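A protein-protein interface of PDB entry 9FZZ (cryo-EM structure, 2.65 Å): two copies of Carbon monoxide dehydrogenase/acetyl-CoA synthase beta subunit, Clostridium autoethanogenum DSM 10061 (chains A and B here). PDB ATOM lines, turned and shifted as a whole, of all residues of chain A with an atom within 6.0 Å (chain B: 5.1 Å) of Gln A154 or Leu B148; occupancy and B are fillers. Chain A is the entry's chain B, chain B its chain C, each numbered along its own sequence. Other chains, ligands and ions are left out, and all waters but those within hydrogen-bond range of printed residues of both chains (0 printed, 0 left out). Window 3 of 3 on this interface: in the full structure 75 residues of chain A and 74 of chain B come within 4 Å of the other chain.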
ATOM      1  N   TYR A 151       0.017  24.403   4.330  1.00  0.00           N
ATOM      2  CA  TYR A 151      -0.327  23.032   3.950  1.00  0.00           C
ATOM      3  C   TYR A 151       0.538  22.487   2.819  1.00  0.00           C
ATOM      4  O   TYR A 151       0.812  21.282   2.797  1.00  0.00           O
ATOM      5  CB  TYR A 151      -1.805  22.945   3.542  1.00  0.00           C
ATOM      6  CG  TYR A 151      -2.725  23.007   4.733  1.00  0.00           C
ATOM      7  CD1 TYR A 151      -3.163  24.235   5.233  1.00  0.00           C
ATOM      8  CD2 TYR A 151      -3.134  21.841   5.386  1.00  0.00           C
ATOM      9  CE1 TYR A 151      -4.003  24.306   6.349  1.00  0.00           C
ATOM     10  CE2 TYR A 151      -3.975  21.895   6.511  1.00  0.00           C
ATOM     11  CZ  TYR A 151      -4.400  23.135   6.977  1.00  0.00           C
ATOM     12  OH  TYR A 151      -5.226  23.240   8.077  1.00  0.00           O
ATOM     13  N   GLY A 152       0.950  23.323   1.867  1.00  0.00           N
ATOM     14  CA  GLY A 152       1.567  22.790   0.667  1.00  0.00           C
ATOM     15  C   GLY A 152       2.788  23.515   0.137  1.00  0.00           C
ATOM     16  O   GLY A 152       3.178  23.287  -1.011  1.00  0.00           O
ATOM     17  N   LYS A 153       3.420  24.363   0.944  1.00  0.00           N
ATOM     18  CA  LYS A 153       4.634  25.043   0.504  1.00  0.00           C
ATOM     19  C   LYS A 153       5.768  24.038   0.324  1.00  0.00           C
ATOM     20  O   LYS A 153       5.972  23.152   1.157  1.00  0.00           O
ATOM     21  CB  LYS A 153       5.036  26.140   1.502  1.00  0.00           C
ATOM     22  CG  LYS A 153       5.352  25.633   2.916  1.00  0.00           C
ATOM     23  CD  LYS A 153       6.515  26.422   3.537  1.00  0.00           C
ATOM     24  CE  LYS A 153       6.217  27.926   3.595  1.00  0.00           C
ATOM     25  NZ  LYS A 153       4.968  28.207   4.391  1.00  0.00           N
ATOM     26  N   GLN A 154       6.521  24.189  -0.769  1.00  0.00           N
ATOM     27  CA  GLN A 154       7.647  23.314  -1.078  1.00  0.00           C
ATOM     28  C   GLN A 154       9.000  23.964  -0.824  1.00  0.00           C
ATOM     29  O   GLN A 154      10.002  23.251  -0.705  1.00  0.00           O
ATOM     30  CB  GLN A 154       7.572  22.854  -2.546  1.00  0.00           C
ATOM     31  CG  GLN A 154       6.221  22.210  -2.910  1.00  0.00           C
ATOM     32  CD  GLN A 154       5.936  20.953  -2.088  1.00  0.00           C
ATOM     33  OE1 GLN A 154       6.778  20.068  -1.991  1.00  0.00           O
ATOM     34  NE2 GLN A 154       4.747  20.877  -1.486  1.00  0.00           N
ATOM     35  N   LEU A 155       9.042  25.286  -0.709  1.00  0.00           N
ATOM     36  CA  LEU A 155      10.251  26.029  -0.391  1.00  0.00           C
ATOM     37  C   LEU A 155      10.014  26.835   0.878  1.00  0.00           C
ATOM     38  O   LEU A 155       8.920  27.362   1.092  1.00  0.00           O
ATOM     39  CB  LEU A 155      10.650  26.971  -1.539  1.00  0.00           C
ATOM     40  CG  LEU A 155      10.951  26.281  -2.879  1.00  0.00           C
ATOM     41  CD1 LEU A 155      11.250  27.305  -3.978  1.00  0.00           C
ATOM     42  CD2 LEU A 155      12.117  25.298  -2.735  1.00  0.00           C
ATOM     43  N   GLY A 156      11.035  26.903   1.729  1.00  0.00           N
ATOM     44  CA  GLY A 156      10.954  27.686   2.945  1.00  0.00           C
ATOM     45  C   GLY A 156      10.438  26.906   4.139  1.00  0.00           C
ATOM     46  O   GLY A 156      10.139  25.710   4.082  1.00  0.00           O
ATOM     47  N   ALA A 181       5.526  21.309   5.386  1.00  0.00           N
ATOM     48  CA  ALA A 181       4.123  21.448   5.004  1.00  0.00           C
ATOM     49  C   ALA A 181       3.356  20.151   5.266  1.00  0.00           C
ATOM     50  O   ALA A 181       3.890  19.050   5.099  1.00  0.00           O
ATOM     51  CB  ALA A 181       4.018  21.859   3.533  1.00  0.00           C
ATOM     52  N   ARG A 184       2.869  17.539   2.561  1.00  0.00           N
ATOM     53  CA  ARG A 184       4.192  17.009   2.247  1.00  0.00           C
ATOM     54  C   ARG A 184       4.612  15.941   3.252  1.00  0.00           C
ATOM     55  O   ARG A 184       5.151  14.901   2.868  1.00  0.00           O
ATOM     56  CB  ARG A 184       5.205  18.162   2.189  1.00  0.00           C
ATOM     57  CG  ARG A 184       6.515  17.835   1.463  1.00  0.00           C
ATOM     58  CD  ARG A 184       7.599  17.405   2.454  1.00  0.00           C
ATOM     59  NE  ARG A 184       8.790  16.914   1.770  1.00  0.00           N
ATOM     60  CZ  ARG A 184       8.890  15.723   1.195  1.00  0.00           C
ATOM     61  NH1 ARG A 184       7.890  14.856   1.209  1.00  0.00           N
ATOM     62  NH2 ARG A 184      10.021  15.394   0.571  1.00  0.00           N
ATOM     63  N   ARG B  97       9.087  15.235  -6.860  1.00  0.00           N
ATOM     64  CA  ARG B  97       9.394  16.402  -6.036  1.00  0.00           C
ATOM     65  C   ARG B  97      10.898  16.572  -5.861  1.00  0.00           C
ATOM     66  O   ARG B  97      11.417  17.693  -5.953  1.00  0.00           O
ATOM     67  CB  ARG B  97       8.707  16.272  -4.671  1.00  0.00           C
ATOM     68  CG  ARG B  97       8.765  17.552  -3.803  1.00  0.00           C
ATOM     69  CD  ARG B  97       8.755  17.215  -2.290  1.00  0.00           C
ATOM     70  NE  ARG B  97       7.833  16.121  -1.993  1.00  0.00           N
ATOM     71  CZ  ARG B  97       6.511  16.238  -1.939  1.00  0.00           C
ATOM     72  NH1 ARG B  97       5.911  17.400  -2.110  1.00  0.00           N
ATOM     73  NH2 ARG B  97       5.770  15.151  -1.720  1.00  0.00           N
ATOM     74  N   ALA B 100      12.183  17.998  -9.070  1.00  0.00           N
ATOM     75  CA  ALA B 100      11.864  19.420  -9.222  1.00  0.00           C
ATOM     76  C   ALA B 100      12.769  20.282  -8.349  1.00  0.00           C
ATOM     77  O   ALA B 100      13.227  21.347  -8.781  1.00  0.00           O
ATOM     78  CB  ALA B 100      10.386  19.675  -8.903  1.00  0.00           C
ATOM     79  N   LEU B 101      13.049  19.841  -7.120  1.00  0.00           N
ATOM     80  CA  LEU B 101      13.974  20.587  -6.264  1.00  0.00           C
ATOM     81  C   LEU B 101      15.375  20.625  -6.878  1.00  0.00           C
ATOM     82  O   LEU B 101      16.038  21.676  -6.883  1.00  0.00           O
ATOM     83  CB  LEU B 101      14.000  19.983  -4.851  1.00  0.00           C
ATOM     84  CG  LEU B 101      12.681  20.143  -4.057  1.00  0.00           C
ATOM     85  CD1 LEU B 101      12.705  19.351  -2.743  1.00  0.00           C
ATOM     86  CD2 LEU B 101      12.355  21.623  -3.769  1.00  0.00           C
ATOM     87  N   TYR B 104      15.362  23.192  -9.441  1.00  0.00           N
ATOM     88  CA  TYR B 104      15.412  24.518  -8.842  1.00  0.00           C
ATOM     89  C   TYR B 104      16.826  24.902  -8.429  1.00  0.00           C
ATOM     90  O   TYR B 104      17.163  26.092  -8.422  1.00  0.00           O
ATOM     91  CB  TYR B 104      14.472  24.568  -7.636  1.00  0.00           C
ATOM     92  CG  TYR B 104      14.347  25.938  -7.033  1.00  0.00           C
ATOM     93  CD1 TYR B 104      13.687  26.967  -7.715  1.00  0.00           C
ATOM     94  CD2 TYR B 104      14.888  26.215  -5.780  1.00  0.00           C
ATOM     95  CE1 TYR B 104      13.576  28.249  -7.155  1.00  0.00           C
ATOM     96  CE2 TYR B 104      14.785  27.484  -5.207  1.00  0.00           C
ATOM     97  CZ  TYR B 104      14.129  28.491  -5.900  1.00  0.00           C
ATOM     98  OH  TYR B 104      14.039  29.737  -5.313  1.00  0.00           O
ATOM     99  N   VAL B 143      10.569  27.336 -14.168  1.00  0.00           N
ATOM    100  CA  VAL B 143       9.908  26.071 -14.469  1.00  0.00           C
ATOM    101  C   VAL B 143       9.838  25.191 -13.230  1.00  0.00           C
ATOM    102  O   VAL B 143       8.809  24.562 -12.948  1.00  0.00           O
ATOM    103  CB  VAL B 143      10.627  25.352 -15.626  1.00  0.00           C
ATOM    104  CG1 VAL B 143      10.130  23.906 -15.751  1.00  0.00           C
ATOM    105  CG2 VAL B 143      10.432  26.125 -16.938  1.00  0.00           C
ATOM    106  N   ALA B 144      10.926  25.132 -12.463  1.00  0.00           N
ATOM    107  CA  ALA B 144      10.919  24.342 -11.236  1.00  0.00           C
ATOM    108  C   ALA B 144       9.907  24.879 -10.231  1.00  0.00           C
ATOM    109  O   ALA B 144       9.215  24.103  -9.564  1.00  0.00           O
ATOM    110  CB  ALA B 144      12.324  24.299 -10.626  1.00  0.00           C
ATOM    111  N   LYS B 145       9.780  26.203 -10.131  1.00  0.00           N
ATOM    112  CA  LYS B 145       8.780  26.795  -9.241  1.00  0.00           C
ATOM    113  C   LYS B 145       7.365  26.392  -9.642  1.00  0.00           C
ATOM    114  O   LYS B 145       6.544  26.027  -8.790  1.00  0.00           O
ATOM    115  CB  LYS B 145       8.913  28.319  -9.218  1.00  0.00           C
ATOM    116  CG  LYS B 145      10.256  28.810  -8.687  1.00  0.00           C
ATOM    117  CD  LYS B 145      10.558  30.199  -9.258  1.00  0.00           C
ATOM    118  CE  LYS B 145      12.045  30.546  -9.169  1.00  0.00           C
ATOM    119  NZ  LYS B 145      12.387  31.729 -10.034  1.00  0.00           N
ATOM    120  N   GLU B 146       7.058  26.447 -10.940  1.00  0.00           N
ATOM    121  CA  GLU B 146       5.726  26.035 -11.394  1.00  0.00           C
ATOM    122  C   GLU B 146       5.475  24.556 -11.102  1.00  0.00           C
ATOM    123  O   GLU B 146       4.398  24.171 -10.614  1.00  0.00           O
ATOM    124  CB  GLU B 146       5.573  26.305 -12.895  1.00  0.00           C
ATOM    125  CG  GLU B 146       5.690  27.777 -13.271  1.00  0.00           C
ATOM    126  CD  GLU B 146       4.658  28.627 -12.548  1.00  0.00           C
ATOM    127  OE1 GLU B 146       3.484  28.216 -12.500  1.00  0.00           O
ATOM    128  OE2 GLU B 146       5.025  29.691 -12.009  1.00  0.00           O
ATOM    129  N   GLY B 147       6.478  23.718 -11.357  1.00  0.00           N
ATOM    130  CA  GLY B 147       6.337  22.299 -11.068  1.00  0.00           C
ATOM    131  C   GLY B 147       6.102  22.019  -9.595  1.00  0.00           C
ATOM    132  O   GLY B 147       5.223  21.237  -9.230  1.00  0.00           O
ATOM    133  N   LEU B 148       6.848  22.705  -8.724  1.00  0.00           N
ATOM    134  CA  LEU B 148       6.662  22.555  -7.282  1.00  0.00           C
ATOM    135  C   LEU B 148       5.278  23.020  -6.854  1.00  0.00           C
ATOM    136  O   LEU B 148       4.641  22.390  -6.004  1.00  0.00           O
ATOM    137  CB  LEU B 148       7.741  23.328  -6.516  1.00  0.00           C
ATOM    138  CG  LEU B 148       9.152  22.722  -6.570  1.00  0.00           C
ATOM    139  CD1 LEU B 148      10.181  23.717  -6.048  1.00  0.00           C
ATOM    140  CD2 LEU B 148       9.227  21.408  -5.789  1.00  0.00           C
ATOM    141  N   SER B 149       4.782  24.102  -7.452  1.00  0.00           N
ATOM    142  CA  SER B 149       3.433  24.554  -7.121  1.00  0.00           C
ATOM    143  C   SER B 149       2.402  23.490  -7.491  1.00  0.00           C
ATOM    144  O   SER B 149       1.399  23.338  -6.789  1.00  0.00           O
ATOM    145  CB  SER B 149       3.131  25.908  -7.782  1.00  0.00           C
ATOM    146  OG  SER B 149       2.832  25.796  -9.166  1.00  0.00           O
ATOM    147  N   ASN B 150       2.662  22.699  -8.540  1.00  0.00           N
ATOM    148  CA  ASN B 150       1.745  21.599  -8.857  1.00  0.00           C
ATOM    149  C   ASN B 150       1.575  20.640  -7.675  1.00  0.00           C
ATOM    150  O   ASN B 150       0.542  19.969  -7.570  1.00  0.00           O
ATOM    151  CB  ASN B 150       2.218  20.809 -10.087  1.00  0.00           C
ATOM    152  CG  ASN B 150       1.478  21.190 -11.369  1.00  0.00           C
ATOM    153  OD1 ASN B 150       0.619  22.063 -11.352  1.00  0.00           O
ATOM    154  ND2 ASN B 150       1.819  20.540 -12.485  1.00  0.00           N
ATOM    155  N   TYR B 151       2.577  20.521  -6.801  1.00  0.00           N
ATOM    156  CA  TYR B 151       2.475  19.550  -5.713  1.00  0.00           C
ATOM    157  C   TYR B 151       1.591  20.031  -4.567  1.00  0.00           C
ATOM    158  O   TYR B 151       0.926  19.206  -3.931  1.00  0.00           O
ATOM    159  CB  TYR B 151       3.869  19.205  -5.170  1.00  0.00           C
ATOM    160  CG  TYR B 151       4.622  18.292  -6.101  1.00  0.00           C
ATOM    161  CD1 TYR B 151       5.396  18.813  -7.139  1.00  0.00           C
ATOM    162  CD2 TYR B 151       4.533  16.904  -5.973  1.00  0.00           C
ATOM    163  CE1 TYR B 151       6.084  17.977  -8.023  1.00  0.00           C
ATOM    164  CE2 TYR B 151       5.217  16.048  -6.854  1.00  0.00           C
ATOM    165  CZ  TYR B 151       5.988  16.602  -7.871  1.00  0.00           C
ATOM    166  OH  TYR B 151       6.677  15.801  -8.760  1.00  0.00           O
ATOM    167  N   GLY B 152       1.586  21.330  -4.266  1.00  0.00           N
ATOM    168  CA  GLY B 152       0.953  21.778  -3.039  1.00  0.00           C
ATOM    169  C   GLY B 152       0.107  23.035  -3.117  1.00  0.00           C
ATOM    170  O   GLY B 152      -0.217  23.611  -2.075  1.00  0.00           O
ATOM    171  N   ASP B 183      -0.053  16.271  -3.397  1.00  0.00           N
ATOM    172  CA  ASP B 183      -0.089  15.975  -1.966  1.00  0.00           C
ATOM    173  C   ASP B 183      -1.490  16.176  -1.397  1.00  0.00           C
ATOM    174  O   ASP B 183      -1.914  15.430  -0.511  1.00  0.00           O
ATOM    175  CB  ASP B 183       0.924  16.841  -1.211  1.00  0.00           C
ATOM    176  CG  ASP B 183       2.361  16.634  -1.677  1.00  0.00           C
ATOM    177  OD1 ASP B 183       2.709  15.505  -2.090  1.00  0.00           O
ATOM    178  OD2 ASP B 183       3.149  17.597  -1.619  1.00  0.00           O
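O of Gly A152 lies within hydrogen-bond range of NE2 of Gln A154, 2.9 Å away. The backbone NH (N) of Arg B97 lies within hydrogen-bond range of the side-chain hydroxyl (OH) of Tyr B151 (3.1 Å). The side-chain carboxylate (OD2) of Asp B183 lies within salt-bridge range of the guanidinium group (NH1) of Arg B97, at 2.8 Å. O of Tyr B151 sits at hydrogen-bond distance from N of Asp B183 (3.1 Å).
Among the printed residues, merely in contact across the chains: Gly A152 with Gly B152 (3.4 Å), Gln A154 with Leu B148 (3.5 Å), Gln A154 with Asp B183 (3.7 Å), Leu A155 with Leu B101 (3.8 Å) and Leu A155 with Tyr B104 (3.7 Å).
Tyr A151 touches none of the printed residues of chain B. Gln A154 touches just these residues of chain B: Arg B97, Leu B148 and Asp B183. Of the printed residues of chain B, Leu A155 touches Leu B101 and Tyr B104. Printed residues of chain A within 4 Å of Leu B101: Leu A155. Of the printed residues of chain A, Tyr B104 touches Leu A155 (3.7 Å). Glu B146 touches none of the printed residues of chain A. Leu B148 touches just one residue of chain A: Gln A154 (3.5 Å). Printed residues of chain A within 4 Å of Asp B183: Gln A154. The nearest residue of chain B that does not touch Gln A154 is Tyr B151 (4.1 Å). The nearest residue of chain A that does not touch Leu B148 is Leu A155 (4.1 Å). The nearest printed residue of chain A that does not touch Arg B97 is Gly A152 (6.6 Å).
The guanidinium group (NH1) of Arg B97 is in hydrogen-bond range of the side-chain amide oxygen (OE1) of Gln A154, 2.8 Å away. The guanidinium group (NH1) of Arg A184 lies close to the guanidinium group (NE) of Arg B97, 3.4 Å away.
Hydrophobic or aromatic side chains of chain A within 4 Å of the printed part of chain B: Leu A155. Along chain A the printed residues that touch a printed residue of chain B span positions 152 to 184. Printed residues of chain B that touch a printed residue of chain A: Arg B97, Leu B101, Tyr B104, Leu B148, Gly B152 and Asp B183. Along chain B the printed residues that touch a printed residue of chain A span positions 97 to 183.
Gly B152 touches its own counterpart, Gly A152. 2 positions are printed for both chains. Of the 7 pairs that touch across the chains among the printed residues, 1 has its exchanged pair printed and touching as well.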
